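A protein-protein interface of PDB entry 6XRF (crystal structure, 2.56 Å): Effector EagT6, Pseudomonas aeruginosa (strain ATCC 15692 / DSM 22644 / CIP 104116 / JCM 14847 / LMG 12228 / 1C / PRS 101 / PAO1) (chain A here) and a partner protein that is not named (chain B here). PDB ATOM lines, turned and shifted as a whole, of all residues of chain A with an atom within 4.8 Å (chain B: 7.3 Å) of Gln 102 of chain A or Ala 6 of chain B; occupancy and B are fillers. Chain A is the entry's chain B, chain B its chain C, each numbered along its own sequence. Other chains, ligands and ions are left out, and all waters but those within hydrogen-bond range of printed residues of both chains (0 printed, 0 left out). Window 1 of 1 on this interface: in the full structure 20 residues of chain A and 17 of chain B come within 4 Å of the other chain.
The backbone carbonyl oxygen of Val 85 of chain A lies within hydrogen-bond range of the backbone NH of Phe 104 of chain A (2.9 Å). N of Leu 87 of chain A lies within hydrogen-bond range of O of Gln 102 of chain A. The side-chain amide oxygen (OE1) of Gln 102 of chain A sits at hydrogen-bond distance from the side-chain hydroxyl (OH) of Tyr 89 of chain A, 2.7 Å away. NE2 of Gln 102 of chain A lies within hydrogen-bond range of OG1 of Thr 115 of chain A (2.6 Å). SD of Met 1 of chain B sits at hydrogen-bond distance from N of Ala 3 of chain B.
Of the 15 printed residues of chain B, 4 touch a printed residue of chain A. Printed residues of chain B that touch a printed residue of chain A: Met 1, Ala 6, Gly 10 and Asp 11. Among the printed residues, no Asp or Glu carboxylate lies within 4 Å of a Lys or Arg side-chain nitrogen of the other chain.
Among the printed residues, pairs that only touch across the chains: Gln 102 of chain A with Met 1 of chain B, Phe 104 of chain A with Met 1 of chain B, Ile 113 of chain A with Met 1 of chain B, Thr 117 of chain A with Asp 11 of chain B and Gln 102 of chain A with Ala 6 of chain B.
The side-chain hydroxyl (OG1) of Thr 117 of chain A lies within hydrogen-bond range of the backbone carbonyl oxygen (O) of Gly 10 of chain B (2.8 Å).
Of the printed residues of chain A, Met 1 of chain B touches Gln 102, Phe 104 and Ile 113. Printed residues of chain B within 4 Å of Thr 117 of chain A: Gly 10 and Asp 11. Printed residues of chain A within 4 Å of Gly 10 of chain B: Thr 117. Of the printed residues of chain B, Ile 113 of chain A touches Met 1. Printed residues of chain A within 4 Å of Asp 11 of chain B: Thr 117 (3.8 Å). Leu 86 of chain A touches none of the printed residues of chain B.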
ATOM      1  N   VAL A  85      24.065 -40.168 -18.066  1.00  0.00           N
ATOM      2  CA  VAL A  85      24.637 -39.646 -16.830  1.00  0.00           C
ATOM      3  C   VAL A  85      23.975 -38.304 -16.545  1.00  0.00           C
ATOM      4  O   VAL A  85      23.827 -37.477 -17.452  1.00  0.00           O
ATOM      5  CB  VAL A  85      26.166 -39.489 -16.938  1.00  0.00           C
ATOM      6  CG1 VAL A  85      26.712 -38.735 -15.735  1.00  0.00           C
ATOM      7  CG2 VAL A  85      26.835 -40.849 -17.078  1.00  0.00           C
ATOM      8  N   LEU A  86      23.566 -38.094 -15.294  1.00  0.00           N
ATOM      9  CA  LEU A  86      22.893 -36.868 -14.889  1.00  0.00           C
ATOM     10  C   LEU A  86      23.755 -36.136 -13.876  1.00  0.00           C
ATOM     11  O   LEU A  86      24.169 -36.724 -12.875  1.00  0.00           O
ATOM     12  CB  LEU A  86      21.512 -37.151 -14.294  1.00  0.00           C
ATOM     13  CG  LEU A  86      20.805 -35.977 -13.604  1.00  0.00           C
ATOM     14  CD1 LEU A  86      19.303 -36.044 -13.875  1.00  0.00           C
ATOM     15  CD2 LEU A  86      21.079 -35.960 -12.103  1.00  0.00           C
ATOM     16  N   LEU A  87      24.001 -34.851 -14.124  1.00  0.00           N
ATOM     17  CA  LEU A  87      24.865 -34.040 -13.278  1.00  0.00           C
ATOM     18  C   LEU A  87      24.082 -32.867 -12.708  1.00  0.00           C
ATOM     19  O   LEU A  87      23.343 -32.197 -13.440  1.00  0.00           O
ATOM     20  CB  LEU A  87      26.078 -33.537 -14.063  1.00  0.00           C
ATOM     21  CG  LEU A  87      26.968 -34.622 -14.666  1.00  0.00           C
ATOM     22  CD1 LEU A  87      27.846 -34.039 -15.763  1.00  0.00           C
ATOM     23  CD2 LEU A  87      27.824 -35.287 -13.607  1.00  0.00           C
ATOM     24  N   TYR A  89      25.275 -29.526 -10.824  1.00  0.00           N
ATOM     25  CA  TYR A  89      26.417 -28.749 -10.364  1.00  0.00           C
ATOM     26  C   TYR A  89      26.098 -27.262 -10.368  1.00  0.00           C
ATOM     27  O   TYR A  89      25.108 -26.808 -10.946  1.00  0.00           O
ATOM     28  CB  TYR A  89      27.678 -29.044 -11.203  1.00  0.00           C
ATOM     29  CG  TYR A  89      27.588 -28.715 -12.667  1.00  0.00           C
ATOM     30  CD1 TYR A  89      27.724 -27.408 -13.115  1.00  0.00           C
ATOM     31  CD2 TYR A  89      27.412 -29.719 -13.612  1.00  0.00           C
ATOM     32  CE1 TYR A  89      27.658 -27.105 -14.459  1.00  0.00           C
ATOM     33  CE2 TYR A  89      27.349 -29.424 -14.955  1.00  0.00           C
ATOM     34  CZ  TYR A  89      27.474 -28.114 -15.372  1.00  0.00           C
ATOM     35  OH  TYR A  89      27.416 -27.802 -16.708  1.00  0.00           O
ATOM     36  N   LEU A 100      22.912 -25.928 -12.577  1.00  0.00           N
ATOM     37  CA  LEU A 100      22.693 -26.651 -13.820  1.00  0.00           C
ATOM     38  C   LEU A 100      22.330 -28.098 -13.521  1.00  0.00           C
ATOM     39  O   LEU A 100      22.921 -28.732 -12.640  1.00  0.00           O
ATOM     40  CB  LEU A 100      23.931 -26.623 -14.719  1.00  0.00           C
ATOM     41  CG  LEU A 100      23.995 -25.507 -15.764  1.00  0.00           C
ATOM     42  CD1 LEU A 100      24.184 -24.156 -15.097  1.00  0.00           C
ATOM     43  CD2 LEU A 100      25.110 -25.789 -16.758  1.00  0.00           C
ATOM     44  N   ARG A 101      21.340 -28.608 -14.245  1.00  0.00           N
ATOM     45  CA  ARG A 101      20.992 -30.025 -14.242  1.00  0.00           C
ATOM     46  C   ARG A 101      21.171 -30.504 -15.675  1.00  0.00           C
ATOM     47  O   ARG A 101      20.429 -30.083 -16.569  1.00  0.00           O
ATOM     48  CB  ARG A 101      19.566 -30.247 -13.743  1.00  0.00           C
ATOM     49  CG  ARG A 101      19.148 -31.714 -13.732  1.00  0.00           C
ATOM     50  CD  ARG A 101      17.954 -31.950 -12.814  1.00  0.00           C
ATOM     51  NE  ARG A 101      18.375 -32.329 -11.460  1.00  0.00           N
ATOM     52  CZ  ARG A 101      17.536 -32.597 -10.464  1.00  0.00           C
ATOM     53  NH1 ARG A 101      16.224 -32.522 -10.657  1.00  0.00           N
ATOM     54  NH2 ARG A 101      18.008 -32.936  -9.277  1.00  0.00           N
ATOM     55  N   GLN A 102      22.161 -31.360 -15.900  1.00  0.00           N
ATOM     56  CA  GLN A 102      22.578 -31.731 -17.246  1.00  0.00           C
ATOM     57  C   GLN A 102      22.589 -33.243 -17.384  1.00  0.00           C
ATOM     58  O   GLN A 102      23.120 -33.946 -16.519  1.00  0.00           O
ATOM     59  CB  GLN A 102      23.965 -31.167 -17.541  1.00  0.00           C
ATOM     60  CG  GLN A 102      24.128 -30.578 -18.904  1.00  0.00           C
ATOM     61  CD  GLN A 102      25.292 -29.621 -18.959  1.00  0.00           C
ATOM     62  OE1 GLN A 102      26.256 -29.763 -18.212  1.00  0.00           O
ATOM     63  NE2 GLN A 102      25.199 -28.623 -19.835  1.00  0.00           N
ATOM     64  N   VAL A 103      22.006 -33.737 -18.470  1.00  0.00           N
ATOM     65  CA  VAL A 103      21.964 -35.162 -18.764  1.00  0.00           C
ATOM     66  C   VAL A 103      22.631 -35.386 -20.113  1.00  0.00           C
ATOM     67  O   VAL A 103      22.289 -34.723 -21.101  1.00  0.00           O
ATOM     68  CB  VAL A 103      20.522 -35.706 -18.763  1.00  0.00           C
ATOM     69  CG1 VAL A 103      20.522 -37.235 -18.880  1.00  0.00           C
ATOM     70  CG2 VAL A 103      19.783 -35.247 -17.504  1.00  0.00           C
ATOM     71  N   PHE A 104      23.586 -36.310 -20.149  1.00  0.00           N
ATOM     72  CA  PHE A 104      24.277 -36.716 -21.367  1.00  0.00           C
ATOM     73  C   PHE A 104      23.740 -38.079 -21.767  1.00  0.00           C
ATOM     74  O   PHE A 104      23.794 -39.022 -20.971  1.00  0.00           O
ATOM     75  CB  PHE A 104      25.791 -36.764 -21.156  1.00  0.00           C
ATOM     76  CG  PHE A 104      26.394 -35.439 -20.777  1.00  0.00           C
ATOM     77  CD1 PHE A 104      26.161 -34.889 -19.526  1.00  0.00           C
ATOM     78  CD2 PHE A 104      27.193 -34.744 -21.667  1.00  0.00           C
ATOM     79  CE1 PHE A 104      26.710 -33.670 -19.177  1.00  0.00           C
ATOM     80  CE2 PHE A 104      27.745 -33.527 -21.321  1.00  0.00           C
ATOM     81  CZ  PHE A 104      27.504 -32.990 -20.076  1.00  0.00           C
ATOM     82  N   ILE A 113      22.592 -33.978 -25.336  1.00  0.00           N
ATOM     83  CA  ILE A 113      22.802 -33.307 -24.058  1.00  0.00           C
ATOM     84  C   ILE A 113      21.560 -32.490 -23.730  1.00  0.00           C
ATOM     85  O   ILE A 113      21.079 -31.715 -24.562  1.00  0.00           O
ATOM     86  CB  ILE A 113      24.048 -32.400 -24.071  1.00  0.00           C
ATOM     87  CG1 ILE A 113      25.285 -33.213 -24.459  1.00  0.00           C
ATOM     88  CG2 ILE A 113      24.251 -31.754 -22.703  1.00  0.00           C
ATOM     89  CD1 ILE A 113      26.567 -32.413 -24.480  1.00  0.00           C
ATOM     90  N   THR A 114      21.048 -32.670 -22.518  1.00  0.00           N
ATOM     91  CA  THR A 114      19.959 -31.874 -21.968  1.00  0.00           C
ATOM     92  C   THR A 114      20.532 -30.996 -20.866  1.00  0.00           C
ATOM     93  O   THR A 114      21.291 -31.484 -20.024  1.00  0.00           O
ATOM     94  CB  THR A 114      18.856 -32.786 -21.424  1.00  0.00           C
ATOM     95  OG1 THR A 114      17.979 -33.175 -22.493  1.00  0.00           O
ATOM     96  CG2 THR A 114      18.072 -32.089 -20.336  1.00  0.00           C
ATOM     97  N   THR A 115      20.183 -29.709 -20.873  1.00  0.00           N
ATOM     98  CA  THR A 115      20.679 -28.780 -19.866  1.00  0.00           C
ATOM     99  C   THR A 115      19.533 -27.924 -19.346  1.00  0.00           C
ATOM    100  O   THR A 115      18.901 -27.195 -20.117  1.00  0.00           O
ATOM    101  CB  THR A 115      21.778 -27.866 -20.426  1.00  0.00           C
ATOM    102  OG1 THR A 115      22.850 -28.641 -20.971  1.00  0.00           O
ATOM    103  CG2 THR A 115      22.333 -26.974 -19.329  1.00  0.00           C
ATOM    104  N   THR A 117      18.910 -24.834 -16.706  1.00  0.00           N
ATOM    105  CA  THR A 117      19.566 -23.794 -15.927  1.00  0.00           C
ATOM    106  C   THR A 117      18.548 -23.148 -15.001  1.00  0.00           C
ATOM    107  O   THR A 117      17.435 -22.822 -15.426  1.00  0.00           O
ATOM    108  CB  THR A 117      20.191 -22.721 -16.822  1.00  0.00           C
ATOM    109  OG1 THR A 117      19.164 -22.087 -17.599  1.00  0.00           O
ATOM    110  CG2 THR A 117      21.233 -23.327 -17.739  1.00  0.00           C
ATOM    111  N   MET B   1      31.536 -30.491 -25.627  1.00  0.00           N
ATOM    112  CA  MET B   1      30.527 -29.476 -25.207  1.00  0.00           C
ATOM    113  C   MET B   1      31.168 -28.400 -24.342  1.00  0.00           C
ATOM    114  O   MET B   1      31.845 -28.700 -23.356  1.00  0.00           O
ATOM    115  CB  MET B   1      29.376 -30.140 -24.446  1.00  0.00           C
ATOM    116  CG  MET B   1      28.386 -29.154 -23.834  1.00  0.00           C
ATOM    117  SD  MET B   1      28.804 -28.667 -22.147  1.00  0.00           S
ATOM    118  CE  MET B   1      27.847 -29.852 -21.206  1.00  0.00           C
ATOM    119  N   ASP B   2      30.944 -27.144 -24.713  1.00  0.00           N
ATOM    120  CA  ASP B   2      31.455 -26.006 -23.954  1.00  0.00           C
ATOM    121  C   ASP B   2      30.491 -25.728 -22.807  1.00  0.00           C
ATOM    122  O   ASP B   2      29.428 -25.133 -23.003  1.00  0.00           O
ATOM    123  CB  ASP B   2      31.611 -24.788 -24.857  1.00  0.00           C
ATOM    124  CG  ASP B   2      32.339 -23.647 -24.172  1.00  0.00           C
ATOM    125  OD1 ASP B   2      32.858 -23.856 -23.055  1.00  0.00           O
ATOM    126  OD2 ASP B   2      32.391 -22.538 -24.749  1.00  0.00           O
ATOM    127  N   ALA B   3      30.857 -26.170 -21.601  1.00  0.00           N
ATOM    128  CA  ALA B   3      30.056 -25.848 -20.425  1.00  0.00           C
ATOM    129  C   ALA B   3      29.952 -24.340 -20.240  1.00  0.00           C
ATOM    130  O   ALA B   3      28.904 -23.826 -19.831  1.00  0.00           O
ATOM    131  CB  ALA B   3      30.662 -26.497 -19.181  1.00  0.00           C
ATOM    132  N   GLN B   4      31.042 -23.622 -20.523  1.00  0.00           N
ATOM    133  CA  GLN B   4      31.028 -22.164 -20.551  1.00  0.00           C
ATOM    134  C   GLN B   4      29.810 -21.627 -21.292  1.00  0.00           C
ATOM    135  O   GLN B   4      29.089 -20.762 -20.783  1.00  0.00           O
ATOM    136  CB  GLN B   4      32.319 -21.678 -21.221  1.00  0.00           C
ATOM    137  CG  GLN B   4      32.840 -20.326 -20.764  1.00  0.00           C
ATOM    138  CD  GLN B   4      34.047 -19.869 -21.578  1.00  0.00           C
ATOM    139  OE1 GLN B   4      34.319 -20.400 -22.657  1.00  0.00           O
ATOM    140  NE2 GLN B   4      34.773 -18.885 -21.062  1.00  0.00           N
ATOM    141  N   ALA B   5      29.565 -22.144 -22.499  1.00  0.00           N
ATOM    142  CA  ALA B   5      28.533 -21.584 -23.367  1.00  0.00           C
ATOM    143  C   ALA B   5      27.145 -22.112 -23.019  1.00  0.00           C
ATOM    144  O   ALA B   5      26.180 -21.339 -22.980  1.00  0.00           O
ATOM    145  CB  ALA B   5      28.863 -21.890 -24.830  1.00  0.00           C
ATOM    146  N   ALA B   6      27.022 -23.420 -22.781  1.00  0.00           N
ATOM    147  CA  ALA B   6      25.733 -23.969 -22.372  1.00  0.00           C
ATOM    148  C   ALA B   6      25.205 -23.250 -21.138  1.00  0.00           C
ATOM    149  O   ALA B   6      24.007 -22.962 -21.041  1.00  0.00           O
ATOM    150  CB  ALA B   6      25.857 -25.469 -22.107  1.00  0.00           C
ATOM    151  N   ALA B   7      26.087 -22.942 -20.186  1.00  0.00           N
ATOM    152  CA  ALA B   7      25.666 -22.189 -19.011  1.00  0.00           C
ATOM    153  C   ALA B   7      25.290 -20.762 -19.389  1.00  0.00           C
ATOM    154  O   ALA B   7      24.248 -20.249 -18.966  1.00  0.00           O
ATOM    155  CB  ALA B   7      26.768 -22.197 -17.954  1.00  0.00           C
ATOM    156  N   ARG B   8      26.129 -20.099 -20.192  1.00  0.00           N
ATOM    157  CA  ARG B   8      25.803 -18.747 -20.631  1.00  0.00           C
ATOM    158  C   ARG B   8      24.483 -18.733 -21.393  1.00  0.00           C
ATOM    159  O   ARG B   8      23.609 -17.898 -21.132  1.00  0.00           O
ATOM    160  CB  ARG B   8      26.937 -18.181 -21.490  1.00  0.00           C
ATOM    161  CG  ARG B   8      26.784 -16.694 -21.829  1.00  0.00           C
ATOM    162  CD  ARG B   8      28.022 -16.126 -22.524  1.00  0.00           C
ATOM    163  NE  ARG B   8      27.700 -14.926 -23.301  1.00  0.00           N
ATOM    164  CZ  ARG B   8      28.587 -14.182 -23.959  1.00  0.00           C
ATOM    165  NH1 ARG B   8      29.876 -14.494 -23.943  1.00  0.00           N
ATOM    166  NH2 ARG B   8      28.183 -13.117 -24.633  1.00  0.00           N
ATOM    167  N   LEU B   9      24.312 -19.668 -22.333  1.00  0.00           N
ATOM    168  CA  LEU B   9      23.096 -19.692 -23.139  1.00  0.00           C
ATOM    169  C   LEU B   9      21.873 -19.943 -22.267  1.00  0.00           C
ATOM    170  O   LEU B   9      20.898 -19.183 -22.310  1.00  0.00           O
ATOM    171  CB  LEU B   9      23.208 -20.759 -24.230  1.00  0.00           C
ATOM    172  CG  LEU B   9      22.172 -20.720 -25.352  1.00  0.00           C
ATOM    173  CD1 LEU B   9      22.024 -19.331 -25.954  1.00  0.00           C
ATOM    174  CD2 LEU B   9      22.558 -21.724 -26.441  1.00  0.00           C
ATOM    175  N   GLY B  10      21.911 -21.006 -21.463  1.00  0.00           N
ATOM    176  CA  GLY B  10      20.781 -21.306 -20.600  1.00  0.00           C
ATOM    177  C   GLY B  10      20.446 -20.165 -19.661  1.00  0.00           C
ATOM    178  O   GLY B  10      19.273 -19.902 -19.382  1.00  0.00           O
ATOM    179  N   ASP B  11      21.469 -19.471 -19.164  1.00  0.00           N
ATOM    180  CA  ASP B  11      21.232 -18.303 -18.323  1.00  0.00           C
ATOM    181  C   ASP B  11      20.590 -17.173 -19.122  1.00  0.00           C
ATOM    182  O   ASP B  11      19.587 -16.589 -18.696  1.00  0.00           O
ATOM    183  CB  ASP B  11      22.548 -17.833 -17.702  1.00  0.00           C
ATOM    184  CG  ASP B  11      22.362 -16.663 -16.766  1.00  0.00           C
ATOM    185  OD1 ASP B  11      21.853 -16.879 -15.647  1.00  0.00           O
ATOM    186  OD2 ASP B  11      22.720 -15.526 -17.146  1.00  0.00           O
ATOM    187  N   GLU B  12      21.156 -16.853 -20.286  1.00  0.00           N
ATOM    188  CA  GLU B  12      20.653 -15.728 -21.066  1.00  0.00           C
ATOM    189  C   GLU B  12      19.192 -15.927 -21.454  1.00  0.00           C
ATOM    190  O   GLU B  12      18.380 -15.004 -21.329  1.00  0.00           O
ATOM    191  CB  GLU B  12      21.519 -15.526 -22.310  1.00  0.00           C
ATOM    192  CG  GLU B  12      22.558 -14.416 -22.154  1.00  0.00           C
ATOM    193  CD  GLU B  12      23.619 -14.434 -23.241  1.00  0.00           C
ATOM    194  OE1 GLU B  12      23.385 -15.065 -24.289  1.00  0.00           O
ATOM    195  OE2 GLU B  12      24.691 -13.822 -23.041  1.00  0.00           O
ATOM    196  N   LEU B  46      25.810 -23.783 -29.947  1.00  0.00           N
ATOM    197  CA  LEU B  46      25.676 -22.956 -28.752  1.00  0.00           C
ATOM    198  C   LEU B  46      26.440 -21.649 -28.911  1.00  0.00           C
ATOM    199  O   LEU B  46      25.873 -20.559 -28.758  1.00  0.00           O
ATOM    200  CB  LEU B  46      26.161 -23.728 -27.528  1.00  0.00           C
ATOM    201  CG  LEU B  46      25.426 -25.037 -27.228  1.00  0.00           C
ATOM    202  CD1 LEU B  46      26.176 -25.857 -26.190  1.00  0.00           C
ATOM    203  CD2 LEU B  46      24.006 -24.758 -26.757  1.00  0.00           C
ATOM    204  N   ALA B  47      27.730 -21.736 -29.243  1.00  0.00           N
ATOM    205  CA  ALA B  47      28.515 -20.529 -29.478  1.00  0.00           C
ATOM    206  C   ALA B  47      27.836 -19.609 -30.488  1.00  0.00           C
ATOM    207  O   ALA B  47      27.799 -18.388 -30.303  1.00  0.00           O
ATOM    208  CB  ALA B  47      29.919 -20.904 -29.957  1.00  0.00           C
ATOM    209  N   ILE B  50      24.787 -17.730 -29.056  1.00  0.00           N
ATOM    210  CA  ILE B  50      25.234 -16.699 -28.120  1.00  0.00           C
ATOM    211  C   ILE B  50      25.652 -15.445 -28.876  1.00  0.00           C
ATOM    212  O   ILE B  50      25.206 -14.333 -28.569  1.00  0.00           O
ATOM    213  CB  ILE B  50      26.374 -17.239 -27.238  1.00  0.00           C
ATOM    214  CG1 ILE B  50      25.797 -18.061 -26.079  1.00  0.00           C
ATOM    215  CG2 ILE B  50      27.237 -16.103 -26.705  1.00  0.00           C
ATOM    216  CD1 ILE B  50      26.743 -19.104 -25.536  1.00  0.00           C
